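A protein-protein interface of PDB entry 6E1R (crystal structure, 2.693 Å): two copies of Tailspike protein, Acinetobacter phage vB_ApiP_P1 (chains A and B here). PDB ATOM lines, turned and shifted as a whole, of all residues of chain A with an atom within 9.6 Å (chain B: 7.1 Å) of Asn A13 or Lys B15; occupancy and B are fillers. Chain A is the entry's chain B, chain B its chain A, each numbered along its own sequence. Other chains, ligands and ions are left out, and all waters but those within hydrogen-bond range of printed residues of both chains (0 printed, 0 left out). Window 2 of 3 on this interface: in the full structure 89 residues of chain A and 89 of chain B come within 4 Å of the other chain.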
ATOM      1  N   MET A  12      -2.823  -6.527  13.944  1.00  0.00           N
ATOM      2  CA  MET A  12      -2.627  -6.760  15.369  1.00  0.00           C
ATOM      3  C   MET A  12      -3.894  -7.317  16.006  1.00  0.00           C
ATOM      4  O   MET A  12      -4.871  -7.601  15.314  1.00  0.00           O
ATOM      5  CB  MET A  12      -2.210  -5.468  16.075  1.00  0.00           C
ATOM      6  CG  MET A  12      -1.053  -5.637  17.045  1.00  0.00           C
ATOM      7  SD  MET A  12      -0.680  -4.026  18.079  1.00  0.00           S
ATOM      8  CE  MET A  12      -1.979  -4.280  19.506  1.00  0.00           C
ATOM      9  N   ASN A  13      -3.873  -7.464  17.329  1.00  0.00           N
ATOM     10  CA  ASN A  13      -5.012  -7.978  18.076  1.00  0.00           C
ATOM     11  C   ASN A  13      -5.163  -7.185  19.365  1.00  0.00           C
ATOM     12  O   ASN A  13      -4.239  -6.496  19.804  1.00  0.00           O
ATOM     13  CB  ASN A  13      -4.843  -9.466  18.410  1.00  0.00           C
ATOM     14  CG  ASN A  13      -5.013 -10.365  17.203  1.00  0.00           C
ATOM     15  OD1 ASN A  13      -5.753 -10.045  16.275  1.00  0.00           O
ATOM     16  ND2 ASN A  13      -4.320 -11.499  17.210  1.00  0.00           N
ATOM     17  N   LEU A  14      -6.344  -7.284  19.971  1.00  0.00           N
ATOM     18  CA  LEU A  14      -6.549  -6.672  21.276  1.00  0.00           C
ATOM     19  C   LEU A  14      -5.778  -7.468  22.322  1.00  0.00           C
ATOM     20  O   LEU A  14      -5.865  -8.700  22.363  1.00  0.00           O
ATOM     21  CB  LEU A  14      -8.036  -6.624  21.622  1.00  0.00           C
ATOM     22  CG  LEU A  14      -8.397  -5.904  22.924  1.00  0.00           C
ATOM     23  CD1 LEU A  14      -8.086  -4.416  22.825  1.00  0.00           C
ATOM     24  CD2 LEU A  14      -9.858  -6.128  23.276  1.00  0.00           C
ATOM     25  N   LYS A  15      -5.021  -6.770  23.170  1.00  0.00           N
ATOM     26  CA  LYS A  15      -4.190  -7.472  24.143  1.00  0.00           C
ATOM     27  C   LYS A  15      -5.039  -8.144  25.216  1.00  0.00           C
ATOM     28  O   LYS A  15      -4.811  -9.309  25.559  1.00  0.00           O
ATOM     29  CB  LYS A  15      -3.180  -6.512  24.770  1.00  0.00           C
ATOM     30  CG  LYS A  15      -2.339  -7.151  25.862  1.00  0.00           C
ATOM     31  CD  LYS A  15      -1.240  -6.230  26.356  1.00  0.00           C
ATOM     32  CE  LYS A  15      -0.444  -6.887  27.473  1.00  0.00           C
ATOM     33  NZ  LYS A  15       0.285  -8.098  27.005  1.00  0.00           N
ATOM     34  N   GLY A  16      -6.016  -7.429  25.758  1.00  0.00           N
ATOM     35  CA  GLY A  16      -6.857  -8.001  26.788  1.00  0.00           C
ATOM     36  C   GLY A  16      -7.725  -6.939  27.432  1.00  0.00           C
ATOM     37  O   GLY A  16      -7.839  -5.815  26.938  1.00  0.00           O
ATOM     38  N   SER A  30       4.235  -4.141  25.357  1.00  0.00           N
ATOM     39  CA  SER A  30       5.170  -3.599  24.383  1.00  0.00           C
ATOM     40  C   SER A  30       4.488  -2.473  23.616  1.00  0.00           C
ATOM     41  O   SER A  30       3.285  -2.240  23.753  1.00  0.00           O
ATOM     42  CB  SER A  30       5.673  -4.687  23.426  1.00  0.00           C
ATOM     43  OG  SER A  30       4.597  -5.343  22.779  1.00  0.00           O
ATOM     44  N   ASP A  31       5.271  -1.780  22.793  1.00  0.00           N
ATOM     45  CA  ASP A  31       4.766  -0.610  22.086  1.00  0.00           C
ATOM     46  C   ASP A  31       3.615  -0.979  21.158  1.00  0.00           C
ATOM     47  O   ASP A  31       3.630  -2.024  20.501  1.00  0.00           O
ATOM     48  CB  ASP A  31       5.889   0.050  21.285  1.00  0.00           C
ATOM     49  CG  ASP A  31       6.807   0.887  22.151  1.00  0.00           C
ATOM     50  OD1 ASP A  31       6.319   1.473  23.141  1.00  0.00           O
ATOM     51  OD2 ASP A  31       8.014   0.961  21.843  1.00  0.00           O
ATOM     52  N   GLY A  32       2.607  -0.106  21.112  1.00  0.00           N
ATOM     53  CA  GLY A  32       1.466  -0.279  20.242  1.00  0.00           C
ATOM     54  C   GLY A  32       0.360  -1.169  20.767  1.00  0.00           C
ATOM     55  O   GLY A  32      -0.737  -1.159  20.194  1.00  0.00           O
ATOM     56  N   GLN A  33       0.599  -1.936  21.829  1.00  0.00           N
ATOM     57  CA  GLN A  33      -0.426  -2.839  22.335  1.00  0.00           C
ATOM     58  C   GLN A  33      -1.574  -2.053  22.956  1.00  0.00           C
ATOM     59  O   GLN A  33      -1.360  -1.066  23.665  1.00  0.00           O
ATOM     60  CB  GLN A  33       0.162  -3.804  23.361  1.00  0.00           C
ATOM     61  CG  GLN A  33       1.166  -4.785  22.788  1.00  0.00           C
ATOM     62  CD  GLN A  33       1.579  -5.838  23.794  1.00  0.00           C
ATOM     63  OE1 GLN A  33       1.664  -5.566  24.991  1.00  0.00           O
ATOM     64  NE2 GLN A  33       1.831  -7.050  23.316  1.00  0.00           N
ATOM     65  N   VAL A  34      -2.799  -2.503  22.694  1.00  0.00           N
ATOM     66  CA  VAL A  34      -4.005  -1.832  23.161  1.00  0.00           C
ATOM     67  C   VAL A  34      -4.759  -2.757  24.106  1.00  0.00           C
ATOM     68  O   VAL A  34      -4.902  -3.954  23.837  1.00  0.00           O
ATOM     69  CB  VAL A  34      -4.905  -1.412  21.979  1.00  0.00           C
ATOM     70  CG1 VAL A  34      -6.078  -0.575  22.468  1.00  0.00           C
ATOM     71  CG2 VAL A  34      -4.096  -0.658  20.935  1.00  0.00           C
ATOM     72  N   VAL A  35      -5.249  -2.191  25.212  1.00  0.00           N
ATOM     73  CA  VAL A  35      -6.033  -2.920  26.199  1.00  0.00           C
ATOM     74  C   VAL A  35      -7.292  -2.119  26.500  1.00  0.00           C
ATOM     75  O   VAL A  35      -7.349  -0.904  26.302  1.00  0.00           O
ATOM     76  CB  VAL A  35      -5.250  -3.190  27.503  1.00  0.00           C
ATOM     77  CG1 VAL A  35      -4.004  -4.006  27.221  1.00  0.00           C
ATOM     78  CG2 VAL A  35      -4.894  -1.883  28.187  1.00  0.00           C
ATOM     79  N   LEU A  36      -8.310  -2.822  26.985  1.00  0.00           N
ATOM     80  CA  LEU A  36      -9.583  -2.218  27.358  1.00  0.00           C
ATOM     81  C   LEU A  36      -9.732  -2.268  28.872  1.00  0.00           C
ATOM     82  O   LEU A  36      -9.756  -3.355  29.460  1.00  0.00           O
ATOM     83  CB  LEU A  36     -10.751  -2.933  26.679  1.00  0.00           C
ATOM     84  CG  LEU A  36     -12.149  -2.585  27.194  1.00  0.00           C
ATOM     85  CD1 LEU A  36     -12.434  -1.099  27.032  1.00  0.00           C
ATOM     86  CD2 LEU A  36     -13.205  -3.420  26.486  1.00  0.00           C
ATOM     87  N   PHE A  51      -6.334   1.811  26.374  1.00  0.00           N
ATOM     88  CA  PHE A  51      -4.972   2.242  26.655  1.00  0.00           C
ATOM     89  C   PHE A  51      -4.002   1.599  25.676  1.00  0.00           C
ATOM     90  O   PHE A  51      -4.086   0.399  25.403  1.00  0.00           O
ATOM     91  CB  PHE A  51      -4.560   1.894  28.093  1.00  0.00           C
ATOM     92  CG  PHE A  51      -5.205   2.758  29.137  1.00  0.00           C
ATOM     93  CD1 PHE A  51      -6.488   2.487  29.582  1.00  0.00           C
ATOM     94  CD2 PHE A  51      -4.531   3.843  29.672  1.00  0.00           C
ATOM     95  CE1 PHE A  51      -7.087   3.282  30.544  1.00  0.00           C
ATOM     96  CE2 PHE A  51      -5.123   4.642  30.634  1.00  0.00           C
ATOM     97  CZ  PHE A  51      -6.403   4.360  31.070  1.00  0.00           C
ATOM     98  N   LYS A  52      -3.077   2.402  25.161  1.00  0.00           N
ATOM     99  CA  LYS A  52      -2.005   1.927  24.299  1.00  0.00           C
ATOM    100  C   LYS A  52      -0.678   2.074  25.028  1.00  0.00           C
ATOM    101  O   LYS A  52      -0.445   3.073  25.713  1.00  0.00           O
ATOM    102  CB  LYS A  52      -1.964   2.694  22.973  1.00  0.00           C
ATOM    103  CG  LYS A  52      -0.898   2.181  22.010  1.00  0.00           C
ATOM    104  CD  LYS A  52      -0.910   2.919  20.681  1.00  0.00           C
ATOM    105  CE  LYS A  52      -2.158   2.596  19.875  1.00  0.00           C
ATOM    106  NZ  LYS A  52      -2.180   3.330  18.580  1.00  0.00           N
ATOM    107  N   TRP A  70       0.971   3.053  29.736  1.00  0.00           N
ATOM    108  CA  TRP A  70      -0.338   2.922  29.108  1.00  0.00           C
ATOM    109  C   TRP A  70      -0.955   4.311  28.988  1.00  0.00           C
ATOM    110  O   TRP A  70      -1.278   4.942  30.001  1.00  0.00           O
ATOM    111  CB  TRP A  70      -1.233   1.996  29.927  1.00  0.00           C
ATOM    112  CG  TRP A  70      -0.699   0.605  30.068  1.00  0.00           C
ATOM    113  CD1 TRP A  70      -0.039   0.088  31.144  1.00  0.00           C
ATOM    114  CD2 TRP A  70      -0.782  -0.451  29.103  1.00  0.00           C
ATOM    115  NE1 TRP A  70       0.295  -1.224  30.911  1.00  0.00           N
ATOM    116  CE2 TRP A  70      -0.150  -1.579  29.664  1.00  0.00           C
ATOM    117  CE3 TRP A  70      -1.329  -0.552  27.821  1.00  0.00           C
ATOM    118  CZ2 TRP A  70      -0.049  -2.792  28.987  1.00  0.00           C
ATOM    119  CZ3 TRP A  70      -1.227  -1.756  27.150  1.00  0.00           C
ATOM    120  CH2 TRP A  70      -0.592  -2.860  27.734  1.00  0.00           C
ATOM    121  N   MET B  12     -18.936 -14.470  17.385  1.00  0.00           N
ATOM    122  CA  MET B  12     -18.159 -13.494  16.627  1.00  0.00           C
ATOM    123  C   MET B  12     -17.052 -12.905  17.494  1.00  0.00           C
ATOM    124  O   MET B  12     -17.310 -12.448  18.606  1.00  0.00           O
ATOM    125  CB  MET B  12     -19.069 -12.382  16.098  1.00  0.00           C
ATOM    126  CG  MET B  12     -18.345 -11.260  15.368  1.00  0.00           C
ATOM    127  SD  MET B  12     -18.247 -11.530  13.439  1.00  0.00           S
ATOM    128  CE  MET B  12     -20.155 -11.534  13.036  1.00  0.00           C
ATOM    129  N   ASN B  13     -15.821 -12.915  16.990  1.00  0.00           N
ATOM    130  CA  ASN B  13     -14.679 -12.386  17.717  1.00  0.00           C
ATOM    131  C   ASN B  13     -14.227 -11.064  17.111  1.00  0.00           C
ATOM    132  O   ASN B  13     -14.569 -10.725  15.975  1.00  0.00           O
ATOM    133  CB  ASN B  13     -13.511 -13.379  17.704  1.00  0.00           C
ATOM    134  CG  ASN B  13     -13.746 -14.570  18.609  1.00  0.00           C
ATOM    135  OD1 ASN B  13     -14.437 -14.469  19.622  1.00  0.00           O
ATOM    136  ND2 ASN B  13     -13.169 -15.710  18.247  1.00  0.00           N
ATOM    137  N   LEU B  14     -13.449 -10.316  17.891  1.00  0.00           N
ATOM    138  CA  LEU B  14     -12.868  -9.075  17.395  1.00  0.00           C
ATOM    139  C   LEU B  14     -11.786  -9.398  16.374  1.00  0.00           C
ATOM    140  O   LEU B  14     -10.920 -10.243  16.620  1.00  0.00           O
ATOM    141  CB  LEU B  14     -12.293  -8.260  18.552  1.00  0.00           C
ATOM    142  CG  LEU B  14     -11.729  -6.874  18.228  1.00  0.00           C
ATOM    143  CD1 LEU B  14     -12.828  -5.938  17.774  1.00  0.00           C
ATOM    144  CD2 LEU B  14     -11.002  -6.297  19.431  1.00  0.00           C
ATOM    145  N   LYS B  15     -11.832  -8.726  15.223  1.00  0.00           N
ATOM    146  CA  LYS B  15     -10.879  -9.039  14.163  1.00  0.00           C
ATOM    147  C   LYS B  15      -9.474  -8.583  14.533  1.00  0.00           C
ATOM    148  O   LYS B  15      -8.503  -9.332  14.369  1.00  0.00           O
ATOM    149  CB  LYS B  15     -11.327  -8.409  12.844  1.00  0.00           C
ATOM    150  CG  LYS B  15     -10.349  -8.635  11.704  1.00  0.00           C
ATOM    151  CD  LYS B  15     -10.904  -8.147  10.382  1.00  0.00           C
ATOM    152  CE  LYS B  15      -9.901  -8.367   9.264  1.00  0.00           C
ATOM    153  NZ  LYS B  15      -9.633  -9.811   9.033  1.00  0.00           N
ATOM    154  N   GLY B  16      -9.345  -7.364  15.039  1.00  0.00           N
ATOM    155  CA  GLY B  16      -8.045  -6.846  15.405  1.00  0.00           C
ATOM    156  C   GLY B  16      -8.135  -5.366  15.713  1.00  0.00           C
ATOM    157  O   GLY B  16      -9.223  -4.810  15.880  1.00  0.00           O
ATOM    158  N   VAL B  17      -6.962  -4.745  15.810  1.00  0.00           N
ATOM    159  CA  VAL B  17      -6.847  -3.323  16.101  1.00  0.00           C
ATOM    160  C   VAL B  17      -5.923  -2.682  15.074  1.00  0.00           C
ATOM    161  O   VAL B  17      -4.879  -3.244  14.723  1.00  0.00           O
ATOM    162  CB  VAL B  17      -6.338  -3.068  17.536  1.00  0.00           C
ATOM    163  CG1 VAL B  17      -7.359  -3.546  18.555  1.00  0.00           C
ATOM    164  CG2 VAL B  17      -5.012  -3.762  17.763  1.00  0.00           C
ATOM    165  N   VAL B  18      -6.323  -1.515  14.573  1.00  0.00           N
ATOM    166  CA  VAL B  18      -5.516  -0.728  13.652  1.00  0.00           C
ATOM    167  C   VAL B  18      -5.293   0.643  14.279  1.00  0.00           C
ATOM    168  O   VAL B  18      -6.055   1.091  15.137  1.00  0.00           O
ATOM    169  CB  VAL B  18      -6.157  -0.606  12.254  1.00  0.00           C
ATOM    170  CG1 VAL B  18      -6.441  -1.984  11.681  1.00  0.00           C
ATOM    171  CG2 VAL B  18      -7.433   0.208  12.323  1.00  0.00           C
ATOM    172  N   LEU B  27      -6.751  -2.746   4.749  1.00  0.00           N
ATOM    173  CA  LEU B  27      -7.083  -3.983   5.443  1.00  0.00           C
ATOM    174  C   LEU B  27      -8.366  -4.584   4.873  1.00  0.00           C
ATOM    175  O   LEU B  27      -9.367  -3.882   4.696  1.00  0.00           O
ATOM    176  CB  LEU B  27      -7.211  -3.722   6.946  1.00  0.00           C
ATOM    177  CG  LEU B  27      -7.446  -4.900   7.895  1.00  0.00           C
ATOM    178  CD1 LEU B  27      -6.711  -4.672   9.204  1.00  0.00           C
ATOM    179  CD2 LEU B  27      -8.920  -5.078   8.171  1.00  0.00           C
ATOM    180  N   SER B  28      -8.332  -5.885   4.596  1.00  0.00           N
ATOM    181  CA  SER B  28      -9.458  -6.606   4.019  1.00  0.00           C
ATOM    182  C   SER B  28     -10.227  -7.360   5.099  1.00  0.00           C
ATOM    183  O   SER B  28      -9.669  -7.751   6.126  1.00  0.00           O
ATOM    184  CB  SER B  28      -8.977  -7.586   2.947  1.00  0.00           C
ATOM    185  OG  SER B  28     -10.070  -8.186   2.274  1.00  0.00           O
ATOM    186  N   GLY B  29     -11.520  -7.563   4.852  1.00  0.00           N
ATOM    187  CA  GLY B  29     -12.365  -8.227   5.825  1.00  0.00           C
ATOM    188  C   GLY B  29     -13.589  -8.850   5.189  1.00  0.00           C
ATOM    189  O   GLY B  29     -13.780  -8.806   3.971  1.00  0.00           O
ATOM    190  N   SER B  30     -14.421  -9.442   6.043  1.00  0.00           N
ATOM    191  CA  SER B  30     -15.666 -10.083   5.646  1.00  0.00           C
ATOM    192  C   SER B  30     -16.833  -9.436   6.383  1.00  0.00           C
ATOM    193  O   SER B  30     -16.649  -8.624   7.292  1.00  0.00           O
ATOM    194  CB  SER B  30     -15.626 -11.591   5.931  1.00  0.00           C
ATOM    195  OG  SER B  30     -14.505 -12.198   5.315  1.00  0.00           O
ATOM    196  N   GLN B  33     -17.536  -8.401  10.446  1.00  0.00           N
ATOM    197  CA  GLN B  33     -16.309  -8.290  11.222  1.00  0.00           C
ATOM    198  C   GLN B  33     -16.148  -6.874  11.757  1.00  0.00           C
ATOM    199  O   GLN B  33     -16.404  -5.892  11.055  1.00  0.00           O
ATOM    200  CB  GLN B  33     -15.100  -8.674  10.371  1.00  0.00           C
ATOM    201  CG  GLN B  33     -15.073 -10.135   9.957  1.00  0.00           C
ATOM    202  CD  GLN B  33     -13.778 -10.521   9.271  1.00  0.00           C
ATOM    203  OE1 GLN B  33     -13.178  -9.720   8.555  1.00  0.00           O
ATOM    204  NE2 GLN B  33     -13.340 -11.756   9.486  1.00  0.00           N
ATOM    205  N   VAL B  34     -15.714  -6.773  13.009  1.00  0.00           N
ATOM    206  CA  VAL B  34     -15.556  -5.496  13.689  1.00  0.00           C
ATOM    207  C   VAL B  34     -14.085  -5.316  14.035  1.00  0.00           C
ATOM    208  O   VAL B  34     -13.416  -6.264  14.460  1.00  0.00           O
ATOM    209  CB  VAL B  34     -16.454  -5.415  14.944  1.00  0.00           C
ATOM    210  CG1 VAL B  34     -15.726  -4.773  16.114  1.00  0.00           C
ATOM    211  CG2 VAL B  34     -17.732  -4.660  14.622  1.00  0.00           C
ATOM    212  N   VAL B  35     -13.584  -4.096  13.842  1.00  0.00           N
ATOM    213  CA  VAL B  35     -12.197  -3.755  14.120  1.00  0.00           C
ATOM    214  C   VAL B  35     -12.172  -2.502  14.987  1.00  0.00           C
ATOM    215  O   VAL B  35     -13.120  -1.715  15.011  1.00  0.00           O
ATOM    216  CB  VAL B  35     -11.393  -3.542  12.814  1.00  0.00           C
ATOM    217  CG1 VAL B  35     -11.814  -2.248  12.130  1.00  0.00           C
ATOM    218  CG2 VAL B  35      -9.892  -3.568  13.069  1.00  0.00           C
ATOM    219  N   LEU B  36     -11.073  -2.334  15.717  1.00  0.00           N
ATOM    220  CA  LEU B  36     -10.861  -1.182  16.585  1.00  0.00           C
ATOM    221  C   LEU B  36      -9.780  -0.296  15.984  1.00  0.00           C
ATOM    222  O   LEU B  36      -8.644  -0.742  15.788  1.00  0.00           O
ATOM    223  CB  LEU B  36     -10.470  -1.621  17.998  1.00  0.00           C
ATOM    224  CG  LEU B  36      -9.910  -0.540  18.930  1.00  0.00           C
ATOM    225  CD1 LEU B  36     -10.894   0.600  19.133  1.00  0.00           C
ATOM    226  CD2 LEU B  36      -9.516  -1.142  20.271  1.00  0.00           C
ATOM    227  N   TYR B  53     -17.531  -4.256   8.838  1.00  0.00           N
ATOM    228  CA  TYR B  53     -17.340  -4.418   7.406  1.00  0.00           C
ATOM    229  C   TYR B  53     -18.669  -4.671   6.707  1.00  0.00           C
ATOM    230  O   TYR B  53     -19.548  -5.360   7.236  1.00  0.00           O
ATOM    231  CB  TYR B  53     -16.373  -5.563   7.117  1.00  0.00           C
ATOM    232  CG  TYR B  53     -15.924  -5.630   5.675  1.00  0.00           C
ATOM    233  CD1 TYR B  53     -16.516  -6.511   4.782  1.00  0.00           C
ATOM    234  CD2 TYR B  53     -14.919  -4.796   5.202  1.00  0.00           C
ATOM    235  CE1 TYR B  53     -16.114  -6.572   3.463  1.00  0.00           C
ATOM    236  CE2 TYR B  53     -14.508  -4.850   3.885  1.00  0.00           C
ATOM    237  CZ  TYR B  53     -15.109  -5.739   3.019  1.00  0.00           C
ATOM    238  OH  TYR B  53     -14.705  -5.797   1.706  1.00  0.00           O
ATOM    239  N   TRP B  70     -15.488  -0.545   5.454  1.00  0.00           N
ATOM    240  CA  TRP B  70     -15.552  -0.420   6.904  1.00  0.00           C
ATOM    241  C   TRP B  70     -16.422   0.780   7.254  1.00  0.00           C
ATOM    242  O   TRP B  70     -16.051   1.926   6.978  1.00  0.00           O
ATOM    243  CB  TRP B  70     -14.150  -0.293   7.491  1.00  0.00           C
ATOM    244  CG  TRP B  70     -13.322  -1.505   7.226  1.00  0.00           C
ATOM    245  CD1 TRP B  70     -12.375  -1.662   6.257  1.00  0.00           C
ATOM    246  CD2 TRP B  70     -13.394  -2.754   7.924  1.00  0.00           C
ATOM    247  NE1 TRP B  70     -11.842  -2.927   6.318  1.00  0.00           N
ATOM    248  CE2 TRP B  70     -12.451  -3.616   7.334  1.00  0.00           C
ATOM    249  CE3 TRP B  70     -14.158  -3.221   8.996  1.00  0.00           C
ATOM    250  CZ2 TRP B  70     -12.256  -4.920   7.778  1.00  0.00           C
ATOM    251  CZ3 TRP B  70     -13.960  -4.514   9.438  1.00  0.00           C
ATOM    252  CH2 TRP B  70     -13.016  -5.349   8.829  1.00  0.00           C
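Printed residues of chain B within 4 Å of Met A12: Gly B16 (3.3 Å) and Val B17 (3.5 Å).
Asn A13 touches two residues of chain B.
Of the printed residues of chain B, Leu A14 touches Leu B14.
Met B12 touches none of the printed residues of chain A.
Of chain A, only Asn A13 comes within 4 Å of Lys B15.
Of chain A, only Met A12 comes within 4 Å of Gly B16.
Printed residues of chain A within 4 Å of Val B17: Met A12 and Asn A13.
The nearest residue of chain A that does not touch Lys B15 is Met A12 (4.1 Å).
The nearest printed residue of chain B that does not touch Met A12 is Lys B15 (4.1 Å).
The backbone carbonyl oxygen (O) of Val B34 lies within hydrogen-bond range of the backbone NH (N) of Lys B15.
The backbone carbonyl oxygen of Gly B16 is in hydrogen-bond range of the backbone NH of Leu B36 (3.1 Å).
The backbone carbonyl oxygen (O) of Lys B15 sits close to the side-chain amide oxygen (OD1) of Asn A13.
Printed residues of chain A that touch a printed residue of chain B: Met A12, Asn A13 and Leu A14.
Hydrophobic or aromatic side chains of chain A within 4 Å of the printed part of chain B: Met A12 and Leu A14.
Of the 17 printed residues of chain B, 4 touch a printed residue of chain A.
Hydrophobic or aromatic side chains of chain B that line the printed part of chain A: Leu B14 and Val B17.
Among the printed residues, pairs that only touch across the chains: Met A12 with Gly B16, Met A12 with Val B17, Asn A13 with Val B17 and Leu A14 with Leu B14.
Met A12 touches Gly B16, but with the chains exchanged Gly A16 does not touch Met B12 (14.0 Å).
Asn A13 touches Lys B15, but with the chains exchanged Lys A15 does not touch Asn B13 (11.8 Å).
Leu A14 touches its own counterpart, Leu B14.
Of the 5 pairs that touch across the chains among the printed residues, 1 has its exchanged pair printed and touching as well.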
